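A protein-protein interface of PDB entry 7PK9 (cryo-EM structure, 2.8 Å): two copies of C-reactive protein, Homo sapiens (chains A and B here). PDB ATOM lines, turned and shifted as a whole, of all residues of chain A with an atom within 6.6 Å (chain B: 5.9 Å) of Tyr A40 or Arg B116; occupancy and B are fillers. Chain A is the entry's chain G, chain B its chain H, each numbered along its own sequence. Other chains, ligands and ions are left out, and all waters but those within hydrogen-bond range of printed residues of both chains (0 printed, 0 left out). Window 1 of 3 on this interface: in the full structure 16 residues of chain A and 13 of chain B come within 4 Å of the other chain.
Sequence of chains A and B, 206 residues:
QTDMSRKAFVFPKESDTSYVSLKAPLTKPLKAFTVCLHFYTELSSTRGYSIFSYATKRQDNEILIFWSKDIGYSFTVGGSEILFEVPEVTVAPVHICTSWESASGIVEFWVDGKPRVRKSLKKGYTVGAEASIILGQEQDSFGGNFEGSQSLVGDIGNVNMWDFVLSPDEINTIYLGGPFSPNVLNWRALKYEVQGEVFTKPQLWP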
ATOM      1  N   HIS A  38       2.326  -8.287  13.325  1.00  0.00           N
ATOM      2  CA  HIS A  38       3.336  -7.232  13.280  1.00  0.00           C
ATOM      3  C   HIS A  38       4.471  -7.549  12.322  1.00  0.00           C
ATOM      4  O   HIS A  38       4.963  -8.675  12.285  1.00  0.00           O
ATOM      5  CB  HIS A  38       3.958  -7.034  14.658  1.00  0.00           C
ATOM      6  CG  HIS A  38       3.242  -6.065  15.531  1.00  0.00           C
ATOM      7  ND1 HIS A  38       3.375  -4.703  15.384  1.00  0.00           N
ATOM      8  CD2 HIS A  38       2.398  -6.253  16.568  1.00  0.00           C
ATOM      9  CE1 HIS A  38       2.638  -4.095  16.291  1.00  0.00           C
ATOM     10  NE2 HIS A  38       2.034  -5.012  17.022  1.00  0.00           N
ATOM     11  N   PHE A  39       4.887  -6.557  11.540  1.00  0.00           N
ATOM     12  CA  PHE A  39       6.145  -6.662  10.819  1.00  0.00           C
ATOM     13  C   PHE A  39       6.865  -5.323  10.753  1.00  0.00           C
ATOM     14  O   PHE A  39       6.259  -4.257  10.851  1.00  0.00           O
ATOM     15  CB  PHE A  39       5.930  -7.263   9.433  1.00  0.00           C
ATOM     16  CG  PHE A  39       5.396  -6.315   8.430  1.00  0.00           C
ATOM     17  CD1 PHE A  39       4.046  -6.052   8.376  1.00  0.00           C
ATOM     18  CD2 PHE A  39       6.229  -5.675   7.552  1.00  0.00           C
ATOM     19  CE1 PHE A  39       3.542  -5.193   7.455  1.00  0.00           C
ATOM     20  CE2 PHE A  39       5.724  -4.812   6.625  1.00  0.00           C
ATOM     21  CZ  PHE A  39       4.379  -4.563   6.584  1.00  0.00           C
ATOM     22  N   TYR A  40       8.185  -5.405  10.620  1.00  0.00           N
ATOM     23  CA  TYR A  40       9.072  -4.247  10.551  1.00  0.00           C
ATOM     24  C   TYR A  40      10.187  -4.424   9.531  1.00  0.00           C
ATOM     25  O   TYR A  40      11.075  -5.255   9.715  1.00  0.00           O
ATOM     26  CB  TYR A  40       9.574  -3.896  11.946  1.00  0.00           C
ATOM     27  CG  TYR A  40      10.273  -2.579  12.004  1.00  0.00           C
ATOM     28  CD1 TYR A  40       9.588  -1.413  11.888  1.00  0.00           C
ATOM     29  CD2 TYR A  40      11.581  -2.502  12.398  1.00  0.00           C
ATOM     30  CE1 TYR A  40      10.218  -0.205  11.973  1.00  0.00           C
ATOM     31  CE2 TYR A  40      12.209  -1.301  12.511  1.00  0.00           C
ATOM     32  CZ  TYR A  40      11.514  -0.153  12.329  1.00  0.00           C
ATOM     33  OH  TYR A  40      12.132   1.058  12.438  1.00  0.00           O
ATOM     34  N   THR A  41      10.126  -3.637   8.455  1.00  0.00           N
ATOM     35  CA  THR A  41      11.032  -3.756   7.322  1.00  0.00           C
ATOM     36  C   THR A  41      11.310  -2.380   6.729  1.00  0.00           C
ATOM     37  O   THR A  41      10.429  -1.524   6.688  1.00  0.00           O
ATOM     38  CB  THR A  41      10.437  -4.684   6.265  1.00  0.00           C
ATOM     39  OG1 THR A  41      11.423  -4.996   5.284  1.00  0.00           O
ATOM     40  CG2 THR A  41       9.260  -4.051   5.604  1.00  0.00           C
ATOM     41  N   GLU A  42      12.556  -2.177   6.294  1.00  0.00           N
ATOM     42  CA  GLU A  42      12.950  -1.048   5.447  1.00  0.00           C
ATOM     43  C   GLU A  42      12.509  -1.176   3.989  1.00  0.00           C
ATOM     44  O   GLU A  42      12.394  -0.158   3.303  1.00  0.00           O
ATOM     45  CB  GLU A  42      14.466  -0.865   5.501  1.00  0.00           C
ATOM     46  CG  GLU A  42      14.961  -0.096   6.713  1.00  0.00           C
ATOM     47  CD  GLU A  42      16.302   0.606   6.478  1.00  0.00           C
ATOM     48  OE1 GLU A  42      17.342   0.108   6.960  1.00  0.00           O
ATOM     49  OE2 GLU A  42      16.312   1.665   5.818  1.00  0.00           O
ATOM     50  N   THR A  90       6.181   4.630   5.787  1.00  0.00           N
ATOM     51  CA  THR A  90       7.198   5.121   6.702  1.00  0.00           C
ATOM     52  C   THR A  90       7.806   3.958   7.474  1.00  0.00           C
ATOM     53  O   THR A  90       7.178   2.914   7.668  1.00  0.00           O
ATOM     54  CB  THR A  90       6.617   6.160   7.681  1.00  0.00           C
ATOM     55  OG1 THR A  90       7.686   6.846   8.345  1.00  0.00           O
ATOM     56  CG2 THR A  90       5.711   5.497   8.716  1.00  0.00           C
ATOM     57  N   VAL A  91       9.055   4.155   7.887  1.00  0.00           N
ATOM     58  CA  VAL A  91       9.811   3.241   8.739  1.00  0.00           C
ATOM     59  C   VAL A  91       9.290   3.157  10.172  1.00  0.00           C
ATOM     60  O   VAL A  91       9.878   3.739  11.087  1.00  0.00           O
ATOM     61  CB  VAL A  91      11.303   3.625   8.729  1.00  0.00           C
ATOM     62  CG1 VAL A  91      12.140   2.548   9.404  1.00  0.00           C
ATOM     63  CG2 VAL A  91      11.801   3.845   7.300  1.00  0.00           C
ATOM     64  N   ALA A  92       8.181   2.449  10.379  1.00  0.00           N
ATOM     65  CA  ALA A  92       7.668   2.180  11.716  1.00  0.00           C
ATOM     66  C   ALA A  92       7.174   0.742  11.706  1.00  0.00           C
ATOM     67  O   ALA A  92       6.649   0.283  10.684  1.00  0.00           O
ATOM     68  CB  ALA A  92       6.533   3.124  12.120  1.00  0.00           C
ATOM     69  N   PRO A  93       7.338  -0.004  12.798  1.00  0.00           N
ATOM     70  CA  PRO A  93       6.535  -1.220  12.962  1.00  0.00           C
ATOM     71  C   PRO A  93       5.070  -0.999  12.643  1.00  0.00           C
ATOM     72  O   PRO A  93       4.450  -0.040  13.105  1.00  0.00           O
ATOM     73  CB  PRO A  93       6.782  -1.624  14.418  1.00  0.00           C
ATOM     74  CG  PRO A  93       7.849  -0.775  14.904  1.00  0.00           C
ATOM     75  CD  PRO A  93       7.908   0.439  14.071  1.00  0.00           C
ATOM     76  N   VAL A  94       4.529  -1.887  11.824  1.00  0.00           N
ATOM     77  CA  VAL A  94       3.157  -1.834  11.338  1.00  0.00           C
ATOM     78  C   VAL A  94       2.402  -3.092  11.750  1.00  0.00           C
ATOM     79  O   VAL A  94       2.878  -4.207  11.522  1.00  0.00           O
ATOM     80  CB  VAL A  94       3.114  -1.606   9.821  1.00  0.00           C
ATOM     81  CG1 VAL A  94       3.638  -2.756   9.115  1.00  0.00           C
ATOM     82  CG2 VAL A  94       1.695  -1.394   9.376  1.00  0.00           C
ATOM     83  N   LEU A 152      10.976 -11.323   2.709  1.00  0.00           N
ATOM     84  CA  LEU A 152      10.994 -10.316   3.761  1.00  0.00           C
ATOM     85  C   LEU A 152      12.393 -10.155   4.337  1.00  0.00           C
ATOM     86  O   LEU A 152      13.100 -11.135   4.578  1.00  0.00           O
ATOM     87  CB  LEU A 152      10.025 -10.695   4.876  1.00  0.00           C
ATOM     88  CG  LEU A 152       9.852  -9.660   5.985  1.00  0.00           C
ATOM     89  CD1 LEU A 152       9.014  -8.496   5.498  1.00  0.00           C
ATOM     90  CD2 LEU A 152       9.247 -10.287   7.209  1.00  0.00           C
ATOM     91  N   VAL A 153      12.784  -8.906   4.566  1.00  0.00           N
ATOM     92  CA  VAL A 153      13.936  -8.549   5.383  1.00  0.00           C
ATOM     93  C   VAL A 153      13.471  -7.670   6.538  1.00  0.00           C
ATOM     94  O   VAL A 153      12.752  -6.690   6.322  1.00  0.00           O
ATOM     95  CB  VAL A 153      15.009  -7.830   4.548  1.00  0.00           C
ATOM     96  CG1 VAL A 153      16.201  -7.471   5.401  1.00  0.00           C
ATOM     97  CG2 VAL A 153      15.434  -8.697   3.382  1.00  0.00           C
ATOM     98  N   GLY A 154      13.890  -8.007   7.759  1.00  0.00           N
ATOM     99  CA  GLY A 154      13.367  -7.391   8.960  1.00  0.00           C
ATOM    100  C   GLY A 154      12.691  -8.397   9.873  1.00  0.00           C
ATOM    101  O   GLY A 154      13.115  -9.554   9.968  1.00  0.00           O
ATOM    102  N   ASP A 155      11.637  -7.945  10.544  1.00  0.00           N
ATOM    103  CA  ASP A 155      11.052  -8.676  11.657  1.00  0.00           C
ATOM    104  C   ASP A 155       9.578  -8.916  11.420  1.00  0.00           C
ATOM    105  O   ASP A 155       8.876  -8.051  10.898  1.00  0.00           O
ATOM    106  CB  ASP A 155      11.195  -7.909  12.966  1.00  0.00           C
ATOM    107  CG  ASP A 155      12.627  -7.691  13.360  1.00  0.00           C
ATOM    108  OD1 ASP A 155      13.462  -8.525  13.000  1.00  0.00           O
ATOM    109  OD2 ASP A 155      12.922  -6.697  14.048  1.00  0.00           O
ATOM    110  N   ILE A 156       9.110 -10.088  11.821  1.00  0.00           N
ATOM    111  CA  ILE A 156       7.694 -10.415  11.790  1.00  0.00           C
ATOM    112  C   ILE A 156       7.351 -11.162  13.070  1.00  0.00           C
ATOM    113  O   ILE A 156       8.148 -11.964  13.558  1.00  0.00           O
ATOM    114  CB  ILE A 156       7.342 -11.234  10.534  1.00  0.00           C
ATOM    115  CG1 ILE A 156       5.844 -11.457  10.449  1.00  0.00           C
ATOM    116  CG2 ILE A 156       8.045 -12.564  10.552  1.00  0.00           C
ATOM    117  CD1 ILE A 156       5.391 -11.777   9.072  1.00  0.00           C
ATOM    118  N   GLY A 157       6.177 -10.887  13.626  1.00  0.00           N
ATOM    119  CA  GLY A 157       5.777 -11.556  14.849  1.00  0.00           C
ATOM    120  C   GLY A 157       4.339 -11.249  15.192  1.00  0.00           C
ATOM    121  O   GLY A 157       3.647 -10.531  14.472  1.00  0.00           O
ATOM    122  N   LEU A 204      10.863  -5.750  18.731  1.00  0.00           N
ATOM    123  CA  LEU A 204      11.258  -4.349  18.844  1.00  0.00           C
ATOM    124  C   LEU A 204      10.073  -3.439  19.130  1.00  0.00           C
ATOM    125  O   LEU A 204      10.202  -2.462  19.874  1.00  0.00           O
ATOM    126  CB  LEU A 204      11.962  -3.889  17.574  1.00  0.00           C
ATOM    127  CG  LEU A 204      13.289  -4.549  17.239  1.00  0.00           C
ATOM    128  CD1 LEU A 204      13.774  -4.055  15.895  1.00  0.00           C
ATOM    129  CD2 LEU A 204      14.311  -4.254  18.313  1.00  0.00           C
ATOM    130  N   TRP A 205       8.920  -3.735  18.546  1.00  0.00           N
ATOM    131  CA  TRP A 205       7.738  -2.940  18.800  1.00  0.00           C
ATOM    132  C   TRP A 205       7.250  -3.118  20.233  1.00  0.00           C
ATOM    133  O   TRP A 205       7.528  -4.131  20.876  1.00  0.00           O
ATOM    134  CB  TRP A 205       6.621  -3.314  17.832  1.00  0.00           C
ATOM    135  CG  TRP A 205       6.452  -4.780  17.640  1.00  0.00           C
ATOM    136  CD1 TRP A 205       5.693  -5.622  18.380  1.00  0.00           C
ATOM    137  CD2 TRP A 205       7.071  -5.577  16.633  1.00  0.00           C
ATOM    138  NE1 TRP A 205       5.819  -6.904  17.915  1.00  0.00           N
ATOM    139  CE2 TRP A 205       6.637  -6.893  16.819  1.00  0.00           C
ATOM    140  CE3 TRP A 205       7.954  -5.301  15.588  1.00  0.00           C
ATOM    141  CZ2 TRP A 205       7.050  -7.928  16.004  1.00  0.00           C
ATOM    142  CZ3 TRP A 205       8.365  -6.330  14.788  1.00  0.00           C
ATOM    143  CH2 TRP A 205       7.910  -7.625  14.991  1.00  0.00           C
ATOM    144  N   TYR B  73      23.787   7.682  10.028  1.00  0.00           N
ATOM    145  CA  TYR B  73      24.706   6.792  10.737  1.00  0.00           C
ATOM    146  C   TYR B  73      25.297   5.654   9.924  1.00  0.00           C
ATOM    147  O   TYR B  73      24.602   4.731   9.503  1.00  0.00           O
ATOM    148  CB  TYR B  73      24.056   6.303  12.027  1.00  0.00           C
ATOM    149  CG  TYR B  73      23.272   7.397  12.693  1.00  0.00           C
ATOM    150  CD1 TYR B  73      23.926   8.359  13.439  1.00  0.00           C
ATOM    151  CD2 TYR B  73      21.904   7.481  12.583  1.00  0.00           C
ATOM    152  CE1 TYR B  73      23.244   9.369  14.054  1.00  0.00           C
ATOM    153  CE2 TYR B  73      21.212   8.493  13.200  1.00  0.00           C
ATOM    154  CZ  TYR B  73      21.886   9.435  13.930  1.00  0.00           C
ATOM    155  OH  TYR B  73      21.198  10.449  14.544  1.00  0.00           O
ATOM    156  N   LEU B  83      24.708   1.291   6.488  1.00  0.00           N
ATOM    157  CA  LEU B  83      24.000   2.553   6.681  1.00  0.00           C
ATOM    158  C   LEU B  83      22.637   2.344   7.334  1.00  0.00           C
ATOM    159  O   LEU B  83      21.886   1.448   6.945  1.00  0.00           O
ATOM    160  CB  LEU B  83      23.821   3.270   5.344  1.00  0.00           C
ATOM    161  CG  LEU B  83      25.054   4.001   4.810  1.00  0.00           C
ATOM    162  CD1 LEU B  83      25.460   5.147   5.716  1.00  0.00           C
ATOM    163  CD2 LEU B  83      26.206   3.045   4.623  1.00  0.00           C
ATOM    164  N   PHE B  84      22.346   3.160   8.344  1.00  0.00           N
ATOM    165  CA  PHE B  84      20.988   3.536   8.772  1.00  0.00           C
ATOM    166  C   PHE B  84      20.582   4.911   8.245  1.00  0.00           C
ATOM    167  O   PHE B  84      20.549   5.907   8.955  1.00  0.00           O
ATOM    168  CB  PHE B  84      20.843   3.414  10.281  1.00  0.00           C
ATOM    169  CG  PHE B  84      21.356   2.127  10.817  1.00  0.00           C
ATOM    170  CD1 PHE B  84      20.513   1.034  10.855  1.00  0.00           C
ATOM    171  CD2 PHE B  84      22.663   1.965  11.188  1.00  0.00           C
ATOM    172  CE1 PHE B  84      20.947  -0.168  11.314  1.00  0.00           C
ATOM    173  CE2 PHE B  84      23.101   0.755  11.645  1.00  0.00           C
ATOM    174  CZ  PHE B  84      22.242  -0.312  11.706  1.00  0.00           C
ATOM    175  N   GLU B  85      20.298   4.942   6.952  1.00  0.00           N
ATOM    176  CA  GLU B  85      19.957   6.176   6.258  1.00  0.00           C
ATOM    177  C   GLU B  85      18.862   6.935   6.996  1.00  0.00           C
ATOM    178  O   GLU B  85      17.754   6.424   7.183  1.00  0.00           O
ATOM    179  CB  GLU B  85      19.460   5.862   4.849  1.00  0.00           C
ATOM    180  CG  GLU B  85      20.454   5.264   3.888  1.00  0.00           C
ATOM    181  CD  GLU B  85      20.674   3.785   4.136  1.00  0.00           C
ATOM    182  OE1 GLU B  85      19.996   3.230   5.025  1.00  0.00           O
ATOM    183  OE2 GLU B  85      21.490   3.168   3.423  1.00  0.00           O
ATOM    184  N   VAL B  86      19.183   8.154   7.420  1.00  0.00           N
ATOM    185  CA  VAL B  86      18.282   8.994   8.204  1.00  0.00           C
ATOM    186  C   VAL B  86      17.712  10.062   7.273  1.00  0.00           C
ATOM    187  O   VAL B  86      18.467  10.935   6.820  1.00  0.00           O
ATOM    188  CB  VAL B  86      19.001   9.644   9.392  1.00  0.00           C
ATOM    189  CG1 VAL B  86      18.063  10.557  10.150  1.00  0.00           C
ATOM    190  CG2 VAL B  86      19.546   8.604  10.313  1.00  0.00           C
ATOM    191  N   PRO B  87      16.411  10.039   6.967  1.00  0.00           N
ATOM    192  CA  PRO B  87      15.866  11.035   6.026  1.00  0.00           C
ATOM    193  C   PRO B  87      15.961  12.480   6.500  1.00  0.00           C
ATOM    194  O   PRO B  87      16.208  13.371   5.677  1.00  0.00           O
ATOM    195  CB  PRO B  87      14.411  10.585   5.859  1.00  0.00           C
ATOM    196  CG  PRO B  87      14.073   9.942   7.145  1.00  0.00           C
ATOM    197  CD  PRO B  87      15.338   9.271   7.626  1.00  0.00           C
ATOM    198  N   VAL B 107      22.963  -6.313  13.959  1.00  0.00           N
ATOM    199  CA  VAL B 107      23.132  -4.954  14.468  1.00  0.00           C
ATOM    200  C   VAL B 107      21.772  -4.359  14.812  1.00  0.00           C
ATOM    201  O   VAL B 107      20.893  -4.283  13.951  1.00  0.00           O
ATOM    202  CB  VAL B 107      23.876  -4.078  13.452  1.00  0.00           C
ATOM    203  CG1 VAL B 107      24.245  -2.757  14.066  1.00  0.00           C
ATOM    204  CG2 VAL B 107      25.122  -4.774  12.961  1.00  0.00           C
ATOM    205  N   GLU B 108      21.584  -3.940  16.059  1.00  0.00           N
ATOM    206  CA  GLU B 108      20.448  -3.094  16.406  1.00  0.00           C
ATOM    207  C   GLU B 108      20.938  -1.664  16.567  1.00  0.00           C
ATOM    208  O   GLU B 108      21.883  -1.407  17.311  1.00  0.00           O
ATOM    209  CB  GLU B 108      19.814  -3.562  17.712  1.00  0.00           C
ATOM    210  CG  GLU B 108      19.044  -4.846  17.628  1.00  0.00           C
ATOM    211  CD  GLU B 108      18.389  -5.212  18.944  1.00  0.00           C
ATOM    212  OE1 GLU B 108      17.983  -6.380  19.103  1.00  0.00           O
ATOM    213  OE2 GLU B 108      18.294  -4.332  19.824  1.00  0.00           O
ATOM    214  N   PHE B 109      20.309  -0.748  15.841  1.00  0.00           N
ATOM    215  CA  PHE B 109      20.458   0.700  15.979  1.00  0.00           C
ATOM    216  C   PHE B 109      19.223   1.364  16.576  1.00  0.00           C
ATOM    217  O   PHE B 109      18.142   1.313  15.985  1.00  0.00           O
ATOM    218  CB  PHE B 109      20.843   1.320  14.644  1.00  0.00           C
ATOM    219  CG  PHE B 109      21.676   2.547  14.787  1.00  0.00           C
ATOM    220  CD1 PHE B 109      21.096   3.774  14.996  1.00  0.00           C
ATOM    221  CD2 PHE B 109      23.048   2.460  14.792  1.00  0.00           C
ATOM    222  CE1 PHE B 109      21.869   4.891  15.143  1.00  0.00           C
ATOM    223  CE2 PHE B 109      23.819   3.574  14.944  1.00  0.00           C
ATOM    224  CZ  PHE B 109      23.229   4.789  15.125  1.00  0.00           C
ATOM    225  N   TRP B 110      19.371   1.979  17.741  1.00  0.00           N
ATOM    226  CA  TRP B 110      18.283   2.682  18.409  1.00  0.00           C
ATOM    227  C   TRP B 110      18.619   4.159  18.421  1.00  0.00           C
ATOM    228  O   TRP B 110      19.703   4.545  18.855  1.00  0.00           O
ATOM    229  CB  TRP B 110      18.129   2.197  19.848  1.00  0.00           C
ATOM    230  CG  TRP B 110      17.647   0.828  19.991  1.00  0.00           C
ATOM    231  CD1 TRP B 110      18.351  -0.310  19.811  1.00  0.00           C
ATOM    232  CD2 TRP B 110      16.332   0.437  20.368  1.00  0.00           C
ATOM    233  NE1 TRP B 110      17.552  -1.397  20.040  1.00  0.00           N
ATOM    234  CE2 TRP B 110      16.309  -0.960  20.400  1.00  0.00           C
ATOM    235  CE3 TRP B 110      15.168   1.137  20.680  1.00  0.00           C
ATOM    236  CZ2 TRP B 110      15.175  -1.670  20.732  1.00  0.00           C
ATOM    237  CZ3 TRP B 110      14.050   0.431  21.013  1.00  0.00           C
ATOM    238  CH2 TRP B 110      14.056  -0.957  21.033  1.00  0.00           C
ATOM    239  N   VAL B 111      17.692   4.977  17.936  1.00  0.00           N
ATOM    240  CA  VAL B 111      17.817   6.429  17.952  1.00  0.00           C
ATOM    241  C   VAL B 111      16.683   7.024  18.767  1.00  0.00           C
ATOM    242  O   VAL B 111      15.510   6.856  18.422  1.00  0.00           O
ATOM    243  CB  VAL B 111      17.817   7.017  16.534  1.00  0.00           C
ATOM    244  CG1 VAL B 111      18.240   8.463  16.559  1.00  0.00           C
ATOM    245  CG2 VAL B 111      18.727   6.225  15.631  1.00  0.00           C
ATOM    246  N   LYS B 114      13.855   4.806  19.585  1.00  0.00           N
ATOM    247  CA  LYS B 114      13.123   4.216  18.481  1.00  0.00           C
ATOM    248  C   LYS B 114      14.027   3.231  17.759  1.00  0.00           C
ATOM    249  O   LYS B 114      15.074   3.649  17.251  1.00  0.00           O
ATOM    250  CB  LYS B 114      12.653   5.316  17.537  1.00  0.00           C
ATOM    251  CG  LYS B 114      11.757   4.861  16.402  1.00  0.00           C
ATOM    252  CD  LYS B 114      10.411   4.375  16.867  1.00  0.00           C
ATOM    253  CE  LYS B 114       9.555   3.997  15.668  1.00  0.00           C
ATOM    254  NZ  LYS B 114      10.112   2.821  14.944  1.00  0.00           N
ATOM    255  N   PRO B 115      13.700   1.943  17.664  1.00  0.00           N
ATOM    256  CA  PRO B 115      14.580   1.028  16.929  1.00  0.00           C
ATOM    257  C   PRO B 115      14.506   1.250  15.426  1.00  0.00           C
ATOM    258  O   PRO B 115      13.422   1.394  14.862  1.00  0.00           O
ATOM    259  CB  PRO B 115      14.049  -0.347  17.328  1.00  0.00           C
ATOM    260  CG  PRO B 115      12.601  -0.121  17.518  1.00  0.00           C
ATOM    261  CD  PRO B 115      12.417   1.301  17.990  1.00  0.00           C
ATOM    262  N   ARG B 116      15.671   1.318  14.784  1.00  0.00           N
ATOM    263  CA  ARG B 116      15.844   0.890  13.401  1.00  0.00           C
ATOM    264  C   ARG B 116      15.669  -0.615  13.228  1.00  0.00           C
ATOM    265  O   ARG B 116      16.007  -1.412  14.103  1.00  0.00           O
ATOM    266  CB  ARG B 116      17.178   1.352  12.840  1.00  0.00           C
ATOM    267  CG  ARG B 116      17.460   2.816  13.086  1.00  0.00           C
ATOM    268  CD  ARG B 116      16.498   3.674  12.287  1.00  0.00           C
ATOM    269  NE  ARG B 116      16.754   3.627  10.854  1.00  0.00           N
ATOM    270  CZ  ARG B 116      17.206   4.629  10.116  1.00  0.00           C
ATOM    271  NH1 ARG B 116      17.281   5.858  10.602  1.00  0.00           N
ATOM    272  NH2 ARG B 116      17.425   4.429   8.828  1.00  0.00           N
ATOM    273  N   VAL B 117      15.157  -0.993  12.062  1.00  0.00           N
ATOM    274  CA  VAL B 117      15.210  -2.363  11.556  1.00  0.00           C
ATOM    275  C   VAL B 117      16.572  -2.986  11.839  1.00  0.00           C
ATOM    276  O   VAL B 117      17.613  -2.360  11.627  1.00  0.00           O
ATOM    277  CB  VAL B 117      14.894  -2.424  10.048  1.00  0.00           C
ATOM    278  CG1 VAL B 117      14.729  -3.853   9.609  1.00  0.00           C
ATOM    279  CG2 VAL B 117      13.630  -1.662   9.701  1.00  0.00           C
ATOM    280  N   ARG B 118      16.554  -4.208  12.371  1.00  0.00           N
ATOM    281  CA  ARG B 118      17.754  -5.024  12.545  1.00  0.00           C
ATOM    282  C   ARG B 118      18.409  -5.420  11.224  1.00  0.00           C
ATOM    283  O   ARG B 118      17.743  -5.857  10.285  1.00  0.00           O
ATOM    284  CB  ARG B 118      17.415  -6.262  13.367  1.00  0.00           C
ATOM    285  CG  ARG B 118      17.403  -5.956  14.842  1.00  0.00           C
ATOM    286  CD  ARG B 118      17.172  -7.160  15.728  1.00  0.00           C
ATOM    287  NE  ARG B 118      15.767  -7.447  15.977  1.00  0.00           N
ATOM    288  CZ  ARG B 118      15.249  -7.726  17.172  1.00  0.00           C
ATOM    289  NH1 ARG B 118      15.955  -7.574  18.279  1.00  0.00           N
ATOM    290  NH2 ARG B 118      13.956  -7.981  17.271  1.00  0.00           N
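Among the printed residues, merely in contact across the chains: Tyr A40 with Val B117 (3.0 Å), Pro A93 with Lys B114 (3.4 Å), Leu A204 with Arg B118 (3.5 Å), Tyr A40 with Arg B116 (3.6 Å), Glu A42 with Val B117 (3.6 Å), Leu A204 with Trp B110 (3.6 Å), Tyr A40 with Lys B114 (3.7 Å), Leu A204 with Pro B115 (3.8 Å), Thr A41 with Val B117 (3.8 Å), Gly A154 with Val B117 (3.8 Å), Leu A204 with Arg B116 (3.9 Å) and Val A91 with Lys B114 (3.97 Å).
Of the 16 printed residues of chain B, 6 touch a printed residue of chain A. Hydrophobic or aromatic side chains of chain B within 4 Å of the printed part of chain A: Trp B110, Pro B115 and Val B117. Among the printed residues, 14 pairs touch across the chains.
The side-chain carboxylate (OD2) of Asp A155 is in salt-bridge range of the guanidinium group (NE) of Arg B118 (3.5 Å). The side-chain hydroxyl of Tyr A40 sits at hydrogen-bond distance from the backbone carbonyl oxygen of Pro B115 (2.8 Å).
No position is printed for both chains.
Printed residues of chain B within 4 Å of Tyr A40: Lys B114, Pro B115, Arg B116 and Val B117. Printed residues of chain B within 4 Å of Glu A42: Val B117 (3.6 Å). Of the printed residues of chain B, Val A91 touches Lys B114. Of the printed residues of chain A, Lys B114 touches Tyr A40, Val A91 and Pro A93. Printed residues of chain B within 4 Å of Pro A93: Lys B114. Printed residues of chain A within 4 Å of Val B117: Tyr A40 (3.0 Å), Thr A41 (3.8 Å), Glu A42 (3.6 Å) and Gly A154 (3.8 Å). The nearest residue of chain A that does not touch Arg B116 is Glu A42 (4.2 Å). The nearest printed residue of chain B that does not touch Asp A155 is Val B117 (5.2 Å).
NH2 of Arg B116 is in hydrogen-bond range of O of Glu B85, at 2.6 Å. The side-chain carboxylate (OE2) of Glu B108 is in hydrogen-bond range of the indole nitrogen (NE1) of Trp B110 (3.0 Å). O of Phe B84 sits close to NH2 of Arg B116 (3.5 Å). O of Phe B109 lies within hydrogen-bond range of N of Arg B116 (2.7 Å). The side-chain carboxylate of Glu B108 is in salt-bridge range of the guanidinium group of Arg B118 (2.5 Å). The backbone NH (N) of Tyr A40 is in hydrogen-bond range of the backbone carbonyl oxygen (O) of Asp A155, at 2.7 Å.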
